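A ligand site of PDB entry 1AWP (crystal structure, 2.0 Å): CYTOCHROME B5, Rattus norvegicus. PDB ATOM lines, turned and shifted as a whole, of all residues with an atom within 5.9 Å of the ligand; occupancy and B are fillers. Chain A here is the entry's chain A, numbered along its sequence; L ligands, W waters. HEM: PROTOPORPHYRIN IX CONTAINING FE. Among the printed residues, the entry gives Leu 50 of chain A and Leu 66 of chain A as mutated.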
ATOM      1  N   MET A  28      14.098   4.769  -9.501  1.00  0.00           N
ATOM      2  CA  MET A  28      13.552   4.756 -10.838  1.00  0.00           C
ATOM      3  C   MET A  28      12.374   5.730 -10.866  1.00  0.00           C
ATOM      4  O   MET A  28      11.649   5.855  -9.875  1.00  0.00           O
ATOM      5  CB  MET A  28      13.075   3.333 -11.156  1.00  0.00           C
ATOM      6  CG  MET A  28      12.406   3.147 -12.492  1.00  0.00           C
ATOM      7  SD  MET A  28      12.076   1.399 -12.748  1.00  0.00           S
ATOM      8  CE  MET A  28      13.666   0.849 -13.304  1.00  0.00           C
ATOM      9  N   ILE A  30       8.753   6.812 -12.534  1.00  0.00           N
ATOM     10  CA  ILE A  30       7.608   6.286 -13.269  1.00  0.00           C
ATOM     11  C   ILE A  30       6.461   7.287 -13.103  1.00  0.00           C
ATOM     12  O   ILE A  30       6.038   7.573 -11.987  1.00  0.00           O
ATOM     13  CB  ILE A  30       7.191   4.896 -12.727  1.00  0.00           C
ATOM     14  CG1 ILE A  30       8.262   3.872 -13.082  1.00  0.00           C
ATOM     15  CG2 ILE A  30       5.871   4.453 -13.346  1.00  0.00           C
ATOM     16  CD1 ILE A  30       7.938   2.469 -12.685  1.00  0.00           C
ATOM     17  N   TYR A  35      10.708   6.137  -7.099  1.00  0.00           N
ATOM     18  CA  TYR A  35      10.561   4.876  -6.376  1.00  0.00           C
ATOM     19  C   TYR A  35      11.900   4.253  -6.059  1.00  0.00           C
ATOM     20  O   TYR A  35      12.777   4.159  -6.909  1.00  0.00           O
ATOM     21  CB  TYR A  35       9.750   3.867  -7.199  1.00  0.00           C
ATOM     22  CG  TYR A  35       8.368   4.334  -7.542  1.00  0.00           C
ATOM     23  CD1 TYR A  35       8.117   5.070  -8.709  1.00  0.00           C
ATOM     24  CD2 TYR A  35       7.295   4.073  -6.690  1.00  0.00           C
ATOM     25  CE1 TYR A  35       6.851   5.537  -8.996  1.00  0.00           C
ATOM     26  CE2 TYR A  35       6.020   4.540  -6.971  1.00  0.00           C
ATOM     27  CZ  TYR A  35       5.802   5.279  -8.127  1.00  0.00           C
ATOM     28  OH  TYR A  35       4.532   5.755  -8.386  1.00  0.00           O
ATOM     29  N   ILE A  37      13.421   1.069  -5.557  1.00  0.00           N
ATOM     30  CA  ILE A  37      13.167  -0.358  -5.791  1.00  0.00           C
ATOM     31  C   ILE A  37      14.362  -1.244  -5.435  1.00  0.00           C
ATOM     32  O   ILE A  37      14.455  -2.379  -5.922  1.00  0.00           O
ATOM     33  CB  ILE A  37      12.790  -0.614  -7.270  1.00  0.00           C
ATOM     34  CG1 ILE A  37      13.922  -0.142  -8.194  1.00  0.00           C
ATOM     35  CG2 ILE A  37      11.504   0.130  -7.617  1.00  0.00           C
ATOM     36  CD1 ILE A  37      13.955  -0.840  -9.538  1.00  0.00           C
ATOM     37  N   PHE A  40      13.328  -4.554  -4.172  1.00  0.00           N
ATOM     38  CA  PHE A  40      12.455  -5.277  -5.078  1.00  0.00           C
ATOM     39  C   PHE A  40      13.226  -5.982  -6.212  1.00  0.00           C
ATOM     40  O   PHE A  40      12.711  -6.889  -6.851  1.00  0.00           O
ATOM     41  CB  PHE A  40      11.433  -4.294  -5.672  1.00  0.00           C
ATOM     42  CG  PHE A  40      10.494  -4.916  -6.668  1.00  0.00           C
ATOM     43  CD1 PHE A  40       9.548  -5.851  -6.271  1.00  0.00           C
ATOM     44  CD2 PHE A  40      10.542  -4.530  -8.003  1.00  0.00           C
ATOM     45  CE1 PHE A  40       8.662  -6.391  -7.194  1.00  0.00           C
ATOM     46  CE2 PHE A  40       9.665  -5.070  -8.932  1.00  0.00           C
ATOM     47  CZ  PHE A  40       8.714  -5.998  -8.525  1.00  0.00           C
ATOM     48  N   HIS A  44      11.294  -9.096  -8.608  1.00  0.00           N
ATOM     49  CA  HIS A  44      10.713  -8.787  -9.905  1.00  0.00           C
ATOM     50  C   HIS A  44      10.593  -9.985 -10.835  1.00  0.00           C
ATOM     51  O   HIS A  44      11.593 -10.544 -11.267  1.00  0.00           O
ATOM     52  CB  HIS A  44      11.507  -7.684 -10.593  1.00  0.00           C
ATOM     53  CG  HIS A  44      10.917  -7.233 -11.885  1.00  0.00           C
ATOM     54  ND1 HIS A  44      11.676  -7.071 -13.030  1.00  0.00           N
ATOM     55  CD2 HIS A  44       9.650  -6.899 -12.224  1.00  0.00           C
ATOM     56  CE1 HIS A  44      10.898  -6.647 -14.004  1.00  0.00           C
ATOM     57  NE2 HIS A  44       9.664  -6.535 -13.539  1.00  0.00           N
ATOM     58  N   PRO A  45       9.374 -10.380 -11.164  1.00  0.00           N
ATOM     59  CA  PRO A  45       9.131 -11.505 -12.059  1.00  0.00           C
ATOM     60  C   PRO A  45       9.836 -11.388 -13.414  1.00  0.00           C
ATOM     61  O   PRO A  45      10.146 -12.392 -14.043  1.00  0.00           O
ATOM     62  CB  PRO A  45       7.610 -11.520 -12.204  1.00  0.00           C
ATOM     63  CG  PRO A  45       7.119 -10.864 -10.960  1.00  0.00           C
ATOM     64  CD  PRO A  45       8.119  -9.791 -10.674  1.00  0.00           C
ATOM     65  N   GLY A  46      10.085 -10.157 -13.845  1.00  0.00           N
ATOM     66  CA  GLY A  46      10.748  -9.943 -15.121  1.00  0.00           C
ATOM     67  C   GLY A  46      12.260  -9.934 -15.039  1.00  0.00           C
ATOM     68  O   GLY A  46      12.938  -9.686 -16.040  1.00  0.00           O
ATOM     69  N   LEU A  50      16.641  -6.091 -16.282  1.00  0.00           N
ATOM     70  CA  LEU A  50      15.872  -5.063 -16.971  1.00  0.00           C
ATOM     71  C   LEU A  50      15.762  -3.809 -16.100  1.00  0.00           C
ATOM     72  O   LEU A  50      15.809  -2.692 -16.605  1.00  0.00           O
ATOM     73  CB  LEU A  50      14.478  -5.592 -17.302  1.00  0.00           C
ATOM     74  CG  LEU A  50      14.413  -6.547 -18.494  1.00  0.00           C
ATOM     75  CD1 LEU A  50      13.073  -7.235 -18.515  1.00  0.00           C
ATOM     76  CD2 LEU A  50      14.640  -5.774 -19.787  1.00  0.00           C
ATOM     77  N   LEU A  51      15.644  -4.017 -14.792  1.00  0.00           N
ATOM     78  CA  LEU A  51      15.526  -2.919 -13.831  1.00  0.00           C
ATOM     79  C   LEU A  51      16.841  -2.127 -13.674  1.00  0.00           C
ATOM     80  O   LEU A  51      16.833  -0.896 -13.679  1.00  0.00           O
ATOM     81  CB  LEU A  51      15.083  -3.450 -12.459  1.00  0.00           C
ATOM     82  CG  LEU A  51      13.708  -4.139 -12.376  1.00  0.00           C
ATOM     83  CD1 LEU A  51      13.429  -4.589 -10.950  1.00  0.00           C
ATOM     84  CD2 LEU A  51      12.626  -3.192 -12.849  1.00  0.00           C
ATOM     85  N   GLN A  54      17.793   0.322 -16.422  1.00  0.00           N
ATOM     86  CA  GLN A  54      17.117   1.615 -16.457  1.00  0.00           C
ATOM     87  C   GLN A  54      17.177   2.328 -15.104  1.00  0.00           C
ATOM     88  O   GLN A  54      16.494   3.331 -14.898  1.00  0.00           O
ATOM     89  CB  GLN A  54      15.666   1.402 -16.881  1.00  0.00           C
ATOM     90  CG  GLN A  54      15.530   0.774 -18.253  1.00  0.00           C
ATOM     91  CD  GLN A  54      14.265   1.216 -18.961  1.00  0.00           C
ATOM     92  OE1 GLN A  54      13.379   0.411 -19.210  1.00  0.00           O
ATOM     93  NE2 GLN A  54      14.169   2.505 -19.271  1.00  0.00           N
ATOM     94  N   ALA A  59      11.534   5.317 -16.307  1.00  0.00           N
ATOM     95  CA  ALA A  59      11.213   4.077 -17.004  1.00  0.00           C
ATOM     96  C   ALA A  59       9.733   3.953 -17.349  1.00  0.00           C
ATOM     97  O   ALA A  59       9.236   2.852 -17.558  1.00  0.00           O
ATOM     98  CB  ALA A  59      11.648   2.891 -16.146  1.00  0.00           C
ATOM     99  N   SER A  62       8.839   2.001 -20.843  1.00  0.00           N
ATOM    100  CA  SER A  62       9.039   0.557 -20.746  1.00  0.00           C
ATOM    101  C   SER A  62       8.016  -0.116 -19.845  1.00  0.00           C
ATOM    102  O   SER A  62       7.468  -1.169 -20.191  1.00  0.00           O
ATOM    103  CB  SER A  62      10.439   0.251 -20.209  1.00  0.00           C
ATOM    104  OG  SER A  62      11.404   1.081 -20.833  1.00  0.00           O
ATOM    105  N   PHE A  63       7.757   0.478 -18.690  1.00  0.00           N
ATOM    106  CA  PHE A  63       6.799  -0.073 -17.750  1.00  0.00           C
ATOM    107  C   PHE A  63       5.437  -0.217 -18.407  1.00  0.00           C
ATOM    108  O   PHE A  63       4.808  -1.282 -18.357  1.00  0.00           O
ATOM    109  CB  PHE A  63       6.681   0.816 -16.503  1.00  0.00           C
ATOM    110  CG  PHE A  63       5.680   0.326 -15.487  1.00  0.00           C
ATOM    111  CD1 PHE A  63       6.073  -0.550 -14.482  1.00  0.00           C
ATOM    112  CD2 PHE A  63       4.361   0.748 -15.525  1.00  0.00           C
ATOM    113  CE1 PHE A  63       5.154  -1.019 -13.539  1.00  0.00           C
ATOM    114  CE2 PHE A  63       3.433   0.291 -14.594  1.00  0.00           C
ATOM    115  CZ  PHE A  63       3.827  -0.599 -13.588  1.00  0.00           C
ATOM    116  N   LEU A  66       5.094  -2.834 -21.661  1.00  0.00           N
ATOM    117  CA  LEU A  66       4.971  -4.254 -21.446  1.00  0.00           C
ATOM    118  C   LEU A  66       3.558  -4.578 -21.007  1.00  0.00           C
ATOM    119  O   LEU A  66       3.169  -5.750 -20.985  1.00  0.00           O
ATOM    120  CB  LEU A  66       5.895  -4.743 -20.358  1.00  0.00           C
ATOM    121  CG  LEU A  66       7.226  -5.147 -20.913  1.00  0.00           C
ATOM    122  CD1 LEU A  66       8.183  -4.666 -19.910  1.00  0.00           C
ATOM    123  CD2 LEU A  66       7.336  -6.668 -21.126  1.00  0.00           C
ATOM    124  N   GLY A  67       2.832  -3.555 -20.623  1.00  0.00           N
ATOM    125  CA  GLY A  67       1.496  -3.814 -20.162  1.00  0.00           C
ATOM    126  C   GLY A  67       1.516  -4.462 -18.786  1.00  0.00           C
ATOM    127  O   GLY A  67       1.155  -5.635 -18.642  1.00  0.00           O
ATOM    128  N   HIS A  68       1.969  -3.724 -17.776  1.00  0.00           N
ATOM    129  CA  HIS A  68       1.970  -4.298 -16.441  1.00  0.00           C
ATOM    130  C   HIS A  68       0.541  -4.373 -15.921  1.00  0.00           C
ATOM    131  O   HIS A  68      -0.317  -3.556 -16.275  1.00  0.00           O
ATOM    132  CB  HIS A  68       2.858  -3.479 -15.498  1.00  0.00           C
ATOM    133  CG  HIS A  68       4.307  -3.760 -15.654  1.00  0.00           C
ATOM    134  ND1 HIS A  68       5.069  -3.177 -16.641  1.00  0.00           N
ATOM    135  CD2 HIS A  68       5.144  -4.584 -14.974  1.00  0.00           C
ATOM    136  CE1 HIS A  68       6.313  -3.623 -16.571  1.00  0.00           C
ATOM    137  NE2 HIS A  68       6.377  -4.479 -15.558  1.00  0.00           N
ATOM    138  N   SER A  69       0.271  -5.361 -15.077  1.00  0.00           N
ATOM    139  CA  SER A  69      -1.069  -5.592 -14.538  1.00  0.00           C
ATOM    140  C   SER A  69      -1.443  -4.640 -13.421  1.00  0.00           C
ATOM    141  O   SER A  69      -0.595  -3.911 -12.886  1.00  0.00           O
ATOM    142  CB  SER A  69      -1.159  -7.024 -14.009  1.00  0.00           C
ATOM    143  OG  SER A  69      -0.528  -7.132 -12.743  1.00  0.00           O
ATOM    144  N   ASP A  71      -2.117  -5.356 -10.556  1.00  0.00           N
ATOM    145  CA  ASP A  71      -1.437  -5.838  -9.360  1.00  0.00           C
ATOM    146  C   ASP A  71      -0.006  -5.319  -9.319  1.00  0.00           C
ATOM    147  O   ASP A  71       0.564  -5.081  -8.253  1.00  0.00           O
ATOM    148  CB  ASP A  71      -1.428  -7.358  -9.323  1.00  0.00           C
ATOM    149  CG  ASP A  71      -2.815  -7.938  -9.220  1.00  0.00           C
ATOM    150  OD1 ASP A  71      -3.534  -7.607  -8.238  1.00  0.00           O
ATOM    151  OD2 ASP A  71      -3.192  -8.724 -10.110  1.00  0.00           O
ATOM    152  N   ALA A  72       0.578  -5.130 -10.498  1.00  0.00           N
ATOM    153  CA  ALA A  72       1.923  -4.601 -10.590  1.00  0.00           C
ATOM    154  C   ALA A  72       1.887  -3.128 -10.176  1.00  0.00           C
ATOM    155  O   ALA A  72       2.776  -2.643  -9.468  1.00  0.00           O
ATOM    156  CB  ALA A  72       2.437  -4.754 -12.021  1.00  0.00           C
ATOM    157  N   ARG A  73       0.849  -2.410 -10.623  1.00  0.00           N
ATOM    158  CA  ARG A  73       0.693  -0.993 -10.271  1.00  0.00           C
ATOM    159  C   ARG A  73       0.526  -0.803  -8.773  1.00  0.00           C
ATOM    160  O   ARG A  73       1.031   0.162  -8.198  1.00  0.00           O
ATOM    161  CB  ARG A  73      -0.522  -0.398 -10.977  1.00  0.00           C
ATOM    162  CG  ARG A  73      -0.293  -0.118 -12.439  1.00  0.00           C
ATOM    163  CD  ARG A  73      -1.562   0.401 -13.084  1.00  0.00           C
ATOM    164  NE  ARG A  73      -1.541   0.205 -14.527  1.00  0.00           N
ATOM    165  CZ  ARG A  73      -0.854   0.966 -15.379  1.00  0.00           C
ATOM    166  NH1 ARG A  73      -0.121   1.971 -14.932  1.00  0.00           N
ATOM    167  NH2 ARG A  73      -0.900   0.708 -16.677  1.00  0.00           N
ATOM    168  N   MET A  75       1.745  -2.689  -6.393  1.00  0.00           N
ATOM    169  CA  MET A  75       3.020  -2.936  -5.739  1.00  0.00           C
ATOM    170  C   MET A  75       3.893  -1.686  -5.676  1.00  0.00           C
ATOM    171  O   MET A  75       4.716  -1.551  -4.772  1.00  0.00           O
ATOM    172  CB  MET A  75       3.789  -4.024  -6.471  1.00  0.00           C
ATOM    173  CG  MET A  75       3.113  -5.369  -6.487  1.00  0.00           C
ATOM    174  SD  MET A  75       4.306  -6.604  -6.980  1.00  0.00           S
ATOM    175  CE  MET A  75       5.514  -6.440  -5.603  1.00  0.00           C
ATOM    176  N   LEU A  76       3.716  -0.784  -6.639  1.00  0.00           N
ATOM    177  CA  LEU A  76       4.505   0.449  -6.690  1.00  0.00           C
ATOM    178  C   LEU A  76       4.359   1.283  -5.415  1.00  0.00           C
ATOM    179  O   LEU A  76       5.321   1.888  -4.928  1.00  0.00           O
ATOM    180  CB  LEU A  76       4.061   1.304  -7.883  1.00  0.00           C
ATOM    181  CG  LEU A  76       4.757   1.081  -9.217  1.00  0.00           C
ATOM    182  CD1 LEU A  76       4.167   2.034 -10.237  1.00  0.00           C
ATOM    183  CD2 LEU A  76       6.255   1.309  -9.068  1.00  0.00           C
ATOM    184  N   TYR A  79       7.071   1.454  -2.731  1.00  0.00           N
ATOM    185  CA  TYR A  79       8.413   1.948  -3.046  1.00  0.00           C
ATOM    186  C   TYR A  79       8.460   3.453  -3.280  1.00  0.00           C
ATOM    187  O   TYR A  79       9.525   4.030  -3.482  1.00  0.00           O
ATOM    188  CB  TYR A  79       8.949   1.190  -4.264  1.00  0.00           C
ATOM    189  CG  TYR A  79       8.926  -0.301  -4.049  1.00  0.00           C
ATOM    190  CD1 TYR A  79       9.753  -0.900  -3.077  1.00  0.00           C
ATOM    191  CD2 TYR A  79       8.051  -1.112  -4.756  1.00  0.00           C
ATOM    192  CE1 TYR A  79       9.697  -2.261  -2.822  1.00  0.00           C
ATOM    193  CE2 TYR A  79       7.980  -2.489  -4.504  1.00  0.00           C
ATOM    194  CZ  TYR A  79       8.804  -3.046  -3.536  1.00  0.00           C
ATOM    195  OH  TYR A  79       8.731  -4.395  -3.287  1.00  0.00           O
HETATM  196  CHA HEM L   1       6.634  -8.547 -15.026  1.00  0.00           C
HETATM  197  CHB HEM L   1       6.266  -5.379 -11.419  1.00  0.00           C
HETATM  198  CHC HEM L   1       9.294  -2.451 -13.736  1.00  0.00           C
HETATM  199  CHD HEM L   1       9.726  -5.644 -17.271  1.00  0.00           C
HETATM  200  C1A HEM L   1       6.236  -7.961 -13.840  1.00  0.00           C
HETATM  201  C2A HEM L   1       5.286  -8.495 -12.872  1.00  0.00           C
HETATM  202  C3A HEM L   1       5.193  -7.618 -11.862  1.00  0.00           C
HETATM  203  C4A HEM L   1       6.063  -6.510 -12.175  1.00  0.00           C
HETATM  204  CMA HEM L   1       4.335  -7.733 -10.598  1.00  0.00           C
HETATM  205  CAA HEM L   1       4.550  -9.844 -13.037  1.00  0.00           C
HETATM  206  CBA HEM L   1       3.360  -9.736 -14.034  1.00  0.00           C
HETATM  207  CGA HEM L   1       2.399  -8.527 -13.849  1.00  0.00           C
HETATM  208  O1A HEM L   1       1.880  -8.421 -12.680  1.00  0.00           O
HETATM  209  O2A HEM L   1       2.199  -7.753 -14.794  1.00  0.00           O
HETATM  210  C1B HEM L   1       7.058  -4.318 -11.721  1.00  0.00           C
HETATM  211  C2B HEM L   1       7.235  -3.137 -10.865  1.00  0.00           C
HETATM  212  C3B HEM L   1       8.077  -2.305 -11.523  1.00  0.00           C
HETATM  213  C4B HEM L   1       8.449  -2.962 -12.760  1.00  0.00           C
HETATM  214  CMB HEM L   1       6.548  -2.911  -9.502  1.00  0.00           C
HETATM  215  CAB HEM L   1       8.587  -0.917 -11.074  1.00  0.00           C
HETATM  216  CBB HEM L   1      10.037  -0.895 -10.568  1.00  0.00           C
HETATM  217  C1C HEM L   1       9.669  -3.065 -14.901  1.00  0.00           C
HETATM  218  C2C HEM L   1      10.597  -2.463 -15.881  1.00  0.00           C
HETATM  219  C3C HEM L   1      10.729  -3.357 -16.872  1.00  0.00           C
HETATM  220  C4C HEM L   1       9.887  -4.504 -16.539  1.00  0.00           C
HETATM  221  CMC HEM L   1      11.261  -1.069 -15.713  1.00  0.00           C
HETATM  222  CAC HEM L   1      11.605  -3.255 -18.147  1.00  0.00           C
HETATM  223  CBC HEM L   1      10.850  -2.966 -19.445  1.00  0.00           C
HETATM  224  C1D HEM L   1       8.935  -6.720 -16.985  1.00  0.00           C
HETATM  225  C2D HEM L   1       8.795  -7.902 -17.807  1.00  0.00           C
HETATM  226  C3D HEM L   1       7.920  -8.726 -17.178  1.00  0.00           C
HETATM  227  C4D HEM L   1       7.522  -8.058 -15.959  1.00  0.00           C
HETATM  228  CMD HEM L   1       9.521  -8.146 -19.151  1.00  0.00           C
HETATM  229  CAD HEM L   1       7.452 -10.093 -17.671  1.00  0.00           C
HETATM  230  CBD HEM L   1       6.099  -9.931 -18.415  1.00  0.00           C
HETATM  231  CGD HEM L   1       5.587 -11.245 -18.917  1.00  0.00           C
HETATM  232  O1D HEM L   1       5.643 -12.249 -18.186  1.00  0.00           O
HETATM  233  O2D HEM L   1       5.135 -11.213 -20.074  1.00  0.00           O
HETATM  234  NA  HEM L   1       6.669  -6.750 -13.396  1.00  0.00           N
HETATM  235  NB  HEM L   1       7.828  -4.184 -12.869  1.00  0.00           N
HETATM  236  NC  HEM L   1       9.239  -4.303 -15.325  1.00  0.00           N
HETATM  237  ND  HEM L   1       8.151  -6.834 -15.839  1.00  0.00           N
HETATM  238 FE   HEM L   1       7.964  -5.538 -14.380  1.00  0.00          FE
HETATM  239  O   HOH W   1       1.349 -10.612 -10.862  1.00  0.00           O
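FE of the ligand is bound by NE2 of His 44 (2.1 Å). FE of the ligand is bound by NE2 of His 68, 2.2 Å away. O2A of the ligand lies within hydrogen-bond range of N of Ser 69 (3.1 Å). The side-chain hydroxyl (OG) of Ser 69 lies within hydrogen-bond range of an oxygen (O1A) of the ligand (2.7 Å).
A ring nitrogen (ND1) of His 68 sits at hydrogen-bond distance from the backbone carbonyl oxygen (O) of Phe 63 (2.6 Å). OG of Ser 69 is in hydrogen-bond range of N of Ala 72. The side-chain hydroxyl (OG) of Ser 69 sits close to the backbone NH (N) of Asp 71, at 3.2 Å. The side-chain amide oxygen of Gln 54 sits at hydrogen-bond distance from the side-chain hydroxyl of Ser 62 (2.6 Å). N of Tyr 35 sits at hydrogen-bond distance from O of Met 28, at 2.9 Å.
Met 28 touches the ligand. Ile 30 touches the ligand (CD1 to CAB, 3.8 Å). CG2 of Ile 37 touches CBB of the ligand (3.5 Å). CE2 of Phe 40 touches C2B of the ligand (3.7 Å). CG of Pro 45 touches CAA of the ligand, at 3.5 Å. Gly 46 touches the ligand. Leu 50 touches the ligand. Leu 51 touches the ligand (CD2 to CHC, 3.5 Å). Ser 62 touches the ligand. Phe 63 touches the ligand. CD1 of Leu 66 touches CBC of the ligand (3.2 Å). Ala 72 touches the ligand. SD of Met 75 touches CMA of the ligand (3.8 Å). Leu 76 touches the ligand. Hydrophobic or aromatic side chains within 4 Å of the ligand: Met 28, Ile 30, Ile 37, Phe 40, His 44, Pro 45, Leu 50, Leu 51, Phe 63, Leu 66, His 68, Ala 72, Met 75 and Leu 76. 17 residues have an atom within 4 Å of the ligand: Met 28, Ile 30, Ile 37, Phe 40, His 44, Pro 45, Gly 46, Leu 50, Leu 51, Ser 62, Phe 63, Leu 66, His 68, Ser 69, Ala 72, Met 75 and Leu 76. Along chain A the residues within 4 Å of the ligand span positions 28 to 76. The nearest printed residue that does not touch the ligand is Ala 59 (4.002 Å).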
